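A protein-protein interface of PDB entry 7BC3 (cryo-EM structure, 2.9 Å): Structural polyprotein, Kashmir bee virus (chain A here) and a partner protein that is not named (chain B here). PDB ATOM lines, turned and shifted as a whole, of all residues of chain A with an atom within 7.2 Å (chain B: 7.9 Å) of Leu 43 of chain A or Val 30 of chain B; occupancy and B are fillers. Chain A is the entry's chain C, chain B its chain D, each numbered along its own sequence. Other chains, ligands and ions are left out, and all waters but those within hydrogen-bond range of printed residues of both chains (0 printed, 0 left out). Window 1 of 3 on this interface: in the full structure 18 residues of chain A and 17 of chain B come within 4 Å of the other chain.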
ATOM      1  N   GLY A  41     -34.715 -13.247 -21.729  1.00  0.00           N
ATOM      2  CA  GLY A  41     -33.969 -14.441 -21.413  1.00  0.00           C
ATOM      3  C   GLY A  41     -32.802 -14.141 -20.495  1.00  0.00           C
ATOM      4  O   GLY A  41     -32.643 -13.039 -19.970  1.00  0.00           O
ATOM      5  N   ASP A  42     -31.969 -15.158 -20.301  1.00  0.00           N
ATOM      6  CA  ASP A  42     -30.770 -14.977 -19.507  1.00  0.00           C
ATOM      7  C   ASP A  42     -29.716 -14.217 -20.312  1.00  0.00           C
ATOM      8  O   ASP A  42     -29.899 -13.897 -21.490  1.00  0.00           O
ATOM      9  CB  ASP A  42     -30.230 -16.326 -19.034  1.00  0.00           C
ATOM     10  CG  ASP A  42     -29.811 -17.223 -20.181  1.00  0.00           C
ATOM     11  OD1 ASP A  42     -30.460 -17.171 -21.245  1.00  0.00           O
ATOM     12  OD2 ASP A  42     -28.832 -17.979 -20.016  1.00  0.00           O
ATOM     13  N   LEU A  43     -28.594 -13.930 -19.655  1.00  0.00           N
ATOM     14  CA  LEU A  43     -27.597 -13.004 -20.169  1.00  0.00           C
ATOM     15  C   LEU A  43     -26.521 -13.677 -21.014  1.00  0.00           C
ATOM     16  O   LEU A  43     -25.416 -13.137 -21.132  1.00  0.00           O
ATOM     17  CB  LEU A  43     -26.944 -12.256 -19.007  1.00  0.00           C
ATOM     18  CG  LEU A  43     -27.786 -11.155 -18.373  1.00  0.00           C
ATOM     19  CD1 LEU A  43     -27.115 -10.635 -17.120  1.00  0.00           C
ATOM     20  CD2 LEU A  43     -28.008 -10.041 -19.362  1.00  0.00           C
ATOM     21  N   ARG A  44     -26.809 -14.830 -21.606  1.00  0.00           N
ATOM     22  CA  ARG A  44     -25.805 -15.507 -22.414  1.00  0.00           C
ATOM     23  C   ARG A  44     -25.690 -14.818 -23.768  1.00  0.00           C
ATOM     24  O   ARG A  44     -26.669 -14.732 -24.517  1.00  0.00           O
ATOM     25  CB  ARG A  44     -26.154 -16.984 -22.583  1.00  0.00           C
ATOM     26  CG  ARG A  44     -25.163 -17.778 -23.444  1.00  0.00           C
ATOM     27  CD  ARG A  44     -23.763 -17.836 -22.832  1.00  0.00           C
ATOM     28  NE  ARG A  44     -23.013 -16.592 -23.028  1.00  0.00           N
ATOM     29  CZ  ARG A  44     -21.786 -16.379 -22.560  1.00  0.00           C
ATOM     30  NH1 ARG A  44     -21.186 -15.219 -22.797  1.00  0.00           N
ATOM     31  NH2 ARG A  44     -21.149 -17.329 -21.879  1.00  0.00           N
ATOM     32  N   ASP A  45     -24.490 -14.322 -24.072  1.00  0.00           N
ATOM     33  CA  ASP A  45     -24.178 -13.706 -25.359  1.00  0.00           C
ATOM     34  C   ASP A  45     -24.856 -12.345 -25.504  1.00  0.00           C
ATOM     35  O   ASP A  45     -25.293 -11.967 -26.591  1.00  0.00           O
ATOM     36  CB  ASP A  45     -24.552 -14.625 -26.522  1.00  0.00           C
ATOM     37  CG  ASP A  45     -23.802 -15.942 -26.486  1.00  0.00           C
ATOM     38  OD1 ASP A  45     -22.598 -15.931 -26.152  1.00  0.00           O
ATOM     39  OD2 ASP A  45     -24.414 -16.988 -26.785  1.00  0.00           O
ATOM     40  N   VAL A  46     -24.941 -11.607 -24.401  1.00  0.00           N
ATOM     41  CA  VAL A  46     -25.351 -10.206 -24.412  1.00  0.00           C
ATOM     42  C   VAL A  46     -24.154  -9.292 -24.187  1.00  0.00           C
ATOM     43  O   VAL A  46     -23.796  -8.498 -25.057  1.00  0.00           O
ATOM     44  CB  VAL A  46     -26.459  -9.941 -23.369  1.00  0.00           C
ATOM     45  CG1 VAL A  46     -26.889  -8.481 -23.405  1.00  0.00           C
ATOM     46  CG2 VAL A  46     -27.646 -10.855 -23.602  1.00  0.00           C
ATOM     47  N   PHE A  47     -23.513  -9.403 -23.041  1.00  0.00           N
ATOM     48  CA  PHE A  47     -22.365  -8.577 -22.726  1.00  0.00           C
ATOM     49  C   PHE A  47     -21.073  -9.311 -23.040  1.00  0.00           C
ATOM     50  O   PHE A  47     -21.048 -10.541 -23.129  1.00  0.00           O
ATOM     51  CB  PHE A  47     -22.387  -8.176 -21.249  1.00  0.00           C
ATOM     52  CG  PHE A  47     -23.582  -7.359 -20.866  1.00  0.00           C
ATOM     53  CD1 PHE A  47     -23.894  -6.205 -21.558  1.00  0.00           C
ATOM     54  CD2 PHE A  47     -24.395  -7.744 -19.818  1.00  0.00           C
ATOM     55  CE1 PHE A  47     -24.990  -5.452 -21.211  1.00  0.00           C
ATOM     56  CE2 PHE A  47     -25.494  -6.993 -19.470  1.00  0.00           C
ATOM     57  CZ  PHE A  47     -25.790  -5.844 -20.167  1.00  0.00           C
ATOM     58  N   SER A  49     -18.801 -10.158 -21.258  1.00  0.00           N
ATOM     59  CA  SER A  49     -18.367 -10.996 -20.151  1.00  0.00           C
ATOM     60  C   SER A  49     -19.580 -11.608 -19.473  1.00  0.00           C
ATOM     61  O   SER A  49     -20.540 -10.899 -19.152  1.00  0.00           O
ATOM     62  CB  SER A  49     -17.553 -10.186 -19.144  1.00  0.00           C
ATOM     63  OG  SER A  49     -16.865 -11.040 -18.253  1.00  0.00           O
ATOM     64  N   ALA A  50     -19.537 -12.920 -19.259  1.00  0.00           N
ATOM     65  CA  ALA A  50     -20.575 -13.629 -18.525  1.00  0.00           C
ATOM     66  C   ALA A  50     -20.441 -13.469 -17.015  1.00  0.00           C
ATOM     67  O   ALA A  50     -21.126 -14.172 -16.266  1.00  0.00           O
ATOM     68  CB  ALA A  50     -20.551 -15.112 -18.895  1.00  0.00           C
ATOM     69  N   VAL A  51     -19.576 -12.568 -16.563  1.00  0.00           N
ATOM     70  CA  VAL A  51     -19.418 -12.287 -15.143  1.00  0.00           C
ATOM     71  C   VAL A  51     -20.485 -11.294 -14.707  1.00  0.00           C
ATOM     72  O   VAL A  51     -20.988 -10.494 -15.503  1.00  0.00           O
ATOM     73  CB  VAL A  51     -18.003 -11.748 -14.858  1.00  0.00           C
ATOM     74  CG1 VAL A  51     -17.819 -10.387 -15.495  1.00  0.00           C
ATOM     75  CG2 VAL A  51     -17.748 -11.664 -13.371  1.00  0.00           C
ATOM     76  N   ASP A  52     -20.835 -11.348 -13.426  1.00  0.00           N
ATOM     77  CA  ASP A  52     -21.762 -10.388 -12.840  1.00  0.00           C
ATOM     78  C   ASP A  52     -20.985  -9.150 -12.415  1.00  0.00           C
ATOM     79  O   ASP A  52     -20.307  -9.158 -11.385  1.00  0.00           O
ATOM     80  CB  ASP A  52     -22.491 -11.012 -11.654  1.00  0.00           C
ATOM     81  CG  ASP A  52     -23.666 -10.182 -11.192  1.00  0.00           C
ATOM     82  OD1 ASP A  52     -24.048  -9.235 -11.911  1.00  0.00           O
ATOM     83  OD2 ASP A  52     -24.209 -10.471 -10.106  1.00  0.00           O
ATOM     84  N   GLU A  53     -21.082  -8.081 -13.199  1.00  0.00           N
ATOM     85  CA  GLU A  53     -20.396  -6.836 -12.883  1.00  0.00           C
ATOM     86  C   GLU A  53     -21.170  -5.965 -11.907  1.00  0.00           C
ATOM     87  O   GLU A  53     -20.723  -4.852 -11.611  1.00  0.00           O
ATOM     88  CB  GLU A  53     -20.131  -6.031 -14.159  1.00  0.00           C
ATOM     89  CG  GLU A  53     -19.133  -6.645 -15.119  1.00  0.00           C
ATOM     90  CD  GLU A  53     -19.773  -7.618 -16.091  1.00  0.00           C
ATOM     91  OE1 GLU A  53     -21.011  -7.787 -16.057  1.00  0.00           O
ATOM     92  OE2 GLU A  53     -19.030  -8.197 -16.909  1.00  0.00           O
ATOM     93  N   VAL B  18     -25.291 -21.423  -7.207  1.00  0.00           N
ATOM     94  CA  VAL B  18     -24.081 -20.636  -7.009  1.00  0.00           C
ATOM     95  C   VAL B  18     -23.340 -21.185  -5.797  1.00  0.00           C
ATOM     96  O   VAL B  18     -23.961 -21.551  -4.792  1.00  0.00           O
ATOM     97  CB  VAL B  18     -24.409 -19.138  -6.828  1.00  0.00           C
ATOM     98  CG1 VAL B  18     -23.160 -18.340  -6.503  1.00  0.00           C
ATOM     99  CG2 VAL B  18     -25.073 -18.584  -8.079  1.00  0.00           C
ATOM    100  N   ARG B  27     -15.359 -13.982  -8.720  1.00  0.00           N
ATOM    101  CA  ARG B  27     -16.336 -13.858  -9.792  1.00  0.00           C
ATOM    102  C   ARG B  27     -17.571 -14.701  -9.501  1.00  0.00           C
ATOM    103  O   ARG B  27     -17.505 -15.725  -8.815  1.00  0.00           O
ATOM    104  CB  ARG B  27     -15.718 -14.291 -11.120  1.00  0.00           C
ATOM    105  CG  ARG B  27     -14.616 -13.378 -11.606  1.00  0.00           C
ATOM    106  CD  ARG B  27     -13.747 -14.061 -12.643  1.00  0.00           C
ATOM    107  NE  ARG B  27     -12.530 -13.302 -12.910  1.00  0.00           N
ATOM    108  CZ  ARG B  27     -11.509 -13.756 -13.629  1.00  0.00           C
ATOM    109  NH1 ARG B  27     -10.442 -12.992 -13.816  1.00  0.00           N
ATOM    110  NH2 ARG B  27     -11.552 -14.970 -14.161  1.00  0.00           N
ATOM    111  N   ILE B  28     -18.704 -14.261 -10.033  1.00  0.00           N
ATOM    112  CA  ILE B  28     -19.958 -14.997  -9.975  1.00  0.00           C
ATOM    113  C   ILE B  28     -20.465 -15.159 -11.402  1.00  0.00           C
ATOM    114  O   ILE B  28     -20.745 -14.161 -12.072  1.00  0.00           O
ATOM    115  CB  ILE B  28     -21.014 -14.290  -9.110  1.00  0.00           C
ATOM    116  CG1 ILE B  28     -20.664 -14.408  -7.633  1.00  0.00           C
ATOM    117  CG2 ILE B  28     -22.376 -14.907  -9.340  1.00  0.00           C
ATOM    118  CD1 ILE B  28     -21.358 -13.397  -6.757  1.00  0.00           C
ATOM    119  N   PRO B  29     -20.598 -16.379 -11.920  1.00  0.00           N
ATOM    120  CA  PRO B  29     -21.242 -16.548 -13.229  1.00  0.00           C
ATOM    121  C   PRO B  29     -22.690 -16.092 -13.178  1.00  0.00           C
ATOM    122  O   PRO B  29     -23.492 -16.597 -12.389  1.00  0.00           O
ATOM    123  CB  PRO B  29     -21.123 -18.053 -13.490  1.00  0.00           C
ATOM    124  CG  PRO B  29     -19.998 -18.499 -12.634  1.00  0.00           C
ATOM    125  CD  PRO B  29     -20.073 -17.655 -11.408  1.00  0.00           C
ATOM    126  N   VAL B  30     -23.023 -15.123 -14.032  1.00  0.00           N
ATOM    127  CA  VAL B  30     -24.369 -14.554 -14.030  1.00  0.00           C
ATOM    128  C   VAL B  30     -25.397 -15.496 -14.631  1.00  0.00           C
ATOM    129  O   VAL B  30     -26.602 -15.265 -14.472  1.00  0.00           O
ATOM    130  CB  VAL B  30     -24.374 -13.210 -14.782  1.00  0.00           C
ATOM    131  CG1 VAL B  30     -24.310 -13.434 -16.281  1.00  0.00           C
ATOM    132  CG2 VAL B  30     -25.591 -12.393 -14.400  1.00  0.00           C
ATOM    133  N   LEU B  31     -24.958 -16.552 -15.314  1.00  0.00           N
ATOM    134  CA  LEU B  31     -25.889 -17.541 -15.843  1.00  0.00           C
ATOM    135  C   LEU B  31     -26.323 -18.535 -14.776  1.00  0.00           C
ATOM    136  O   LEU B  31     -27.415 -19.105 -14.873  1.00  0.00           O
ATOM    137  CB  LEU B  31     -25.252 -18.275 -17.020  1.00  0.00           C
ATOM    138  CG  LEU B  31     -24.721 -17.351 -18.113  1.00  0.00           C
ATOM    139  CD1 LEU B  31     -23.956 -18.132 -19.158  1.00  0.00           C
ATOM    140  CD2 LEU B  31     -25.863 -16.581 -18.745  1.00  0.00           C
ATOM    141  N   GLY B  32     -25.487 -18.761 -13.767  1.00  0.00           N
ATOM    142  CA  GLY B  32     -25.880 -19.579 -12.639  1.00  0.00           C
ATOM    143  C   GLY B  32     -26.747 -18.872 -11.626  1.00  0.00           C
ATOM    144  O   GLY B  32     -27.221 -19.508 -10.681  1.00  0.00           O
ATOM    145  N   GLU B  33     -26.958 -17.565 -11.796  1.00  0.00           N
ATOM    146  CA  GLU B  33     -27.838 -16.833 -10.894  1.00  0.00           C
ATOM    147  C   GLU B  33     -29.303 -17.138 -11.175  1.00  0.00           C
ATOM    148  O   GLU B  33     -30.140 -17.013 -10.274  1.00  0.00           O
ATOM    149  CB  GLU B  33     -27.569 -15.334 -11.014  1.00  0.00           C
ATOM    150  CG  GLU B  33     -26.149 -14.938 -10.667  1.00  0.00           C
ATOM    151  CD  GLU B  33     -25.952 -13.438 -10.648  1.00  0.00           C
ATOM    152  OE1 GLU B  33     -26.890 -12.709 -11.028  1.00  0.00           O
ATOM    153  OE2 GLU B  33     -24.857 -12.991 -10.251  1.00  0.00           O
ATOM    154  N   ILE B  34     -29.632 -17.545 -12.400  1.00  0.00           N
ATOM    155  CA  ILE B  34     -30.987 -17.956 -12.751  1.00  0.00           C
ATOM    156  C   ILE B  34     -30.920 -18.825 -13.999  1.00  0.00           C
ATOM    157  O   ILE B  34     -29.996 -18.717 -14.810  1.00  0.00           O
ATOM    158  CB  ILE B  34     -31.934 -16.754 -12.977  1.00  0.00           C
ATOM    159  CG1 ILE B  34     -33.387 -17.234 -13.071  1.00  0.00           C
ATOM    160  CG2 ILE B  34     -31.533 -16.013 -14.250  1.00  0.00           C
ATOM    161  CD1 ILE B  34     -33.953 -17.827 -11.803  1.00  0.00           C
ATOM    162  N   ALA B  35     -31.920 -19.688 -14.148  1.00  0.00           N
ATOM    163  CA  ALA B  35     -32.091 -20.538 -15.321  1.00  0.00           C
ATOM    164  C   ALA B  35     -33.233 -19.965 -16.151  1.00  0.00           C
ATOM    165  O   ALA B  35     -34.405 -20.142 -15.814  1.00  0.00           O
ATOM    166  CB  ALA B  35     -32.375 -21.981 -14.911  1.00  0.00           C
ATOM    167  N   LYS B  36     -32.886 -19.276 -17.234  1.00  0.00           N
ATOM    168  CA  LYS B  36     -33.875 -18.784 -18.181  1.00  0.00           C
ATOM    169  C   LYS B  36     -33.352 -18.957 -19.602  1.00  0.00           C
ATOM    170  O   LYS B  36     -33.329 -17.994 -20.379  1.00  0.00           O
ATOM    171  CB  LYS B  36     -34.209 -17.318 -17.904  1.00  0.00           C
ATOM    172  CG  LYS B  36     -35.245 -17.109 -16.817  1.00  0.00           C
ATOM    173  CD  LYS B  36     -35.960 -15.776 -16.975  1.00  0.00           C
ATOM    174  CE  LYS B  36     -35.035 -14.611 -16.659  1.00  0.00           C
ATOM    175  NZ  LYS B  36     -35.588 -13.314 -17.134  1.00  0.00           N
ATOM    176  N   PRO B  37     -32.921 -20.161 -19.979  1.00  0.00           N
ATOM    177  CA  PRO B  37     -32.441 -20.374 -21.348  1.00  0.00           C
ATOM    178  C   PRO B  37     -33.589 -20.487 -22.334  1.00  0.00           C
ATOM    179  O   PRO B  37     -34.746 -20.244 -21.974  1.00  0.00           O
ATOM    180  CB  PRO B  37     -31.657 -21.684 -21.234  1.00  0.00           C
ATOM    181  CG  PRO B  37     -32.369 -22.431 -20.174  1.00  0.00           C
ATOM    182  CD  PRO B  37     -32.909 -21.411 -19.201  1.00  0.00           C
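The backbone NH (N) of Asp 52 of chain A sits at hydrogen-bond distance from the backbone carbonyl oxygen (O) of Ile 28 of chain B, 3.1 Å away.
O of Ala 50 of chain A sits at hydrogen-bond distance from N of Val 30 of chain B, 3.1 Å away.
The side-chain carboxylate of Asp 52 of chain A sits close to the side-chain carboxylate of Glu 33 of chain B (2.6 Å).
The backbone carbonyl oxygen (O) of Lys 36 of chain B sits at hydrogen-bond distance from the backbone NH (N) of Asp 42 of chain A, at 3.1 Å.
NE of Arg 44 of chain A is in salt-bridge range of OD1 of Asp 45 of chain A (3.2 Å).
Among the printed residues, merely in contact across the chains: Arg 44 of chain A with Leu 31 of chain B, Asp 42 of chain A with Leu 31 of chain B, Leu 43 of chain A with Val 30 of chain B, Leu 43 of chain A with Leu 31 of chain B, Gly 41 of chain A with Lys 36 of chain B, Asp 42 of chain A with Pro 37 of chain B, Val 51 of chain A with Ile 28 of chain B, Ala 50 of chain A with Pro 29 of chain B and Val 51 of chain A with Arg 27 of chain B.
Of chain B, only Val 30 (3.6 Å) and Leu 31 (3.7 Å) come within 4 Å of Leu 43 of chain A.
Of the printed residues of chain A, Val 30 of chain B touches Leu 43 (3.6 Å) and Ala 50 (3.1 Å).
Of the printed residues of chain B, Gly 41 of chain A touches Lys 36.
Of the printed residues of chain B, Asp 42 of chain A touches Leu 31 (3.5 Å), Lys 36 (3.1 Å) and Pro 37 (3.8 Å).
Of the printed residues of chain A, Pro 37 of chain B touches Asp 42.
Of the printed residues of chain B, Arg 44 of chain A touches Leu 31.
Of the printed residues of chain A, Leu 31 of chain B touches Asp 42, Leu 43 and Arg 44.
Asp 45 of chain A touches none of the printed residues of chain B.
The nearest residue of chain B that does not touch Leu 43 of chain A is Lys 36 of chain B (6.3 Å).
The nearest residue of chain A that does not touch Val 30 of chain B is Asp 52 of chain A (4.2 Å).
Among the printed residues, 13 pairs touch across the chains.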
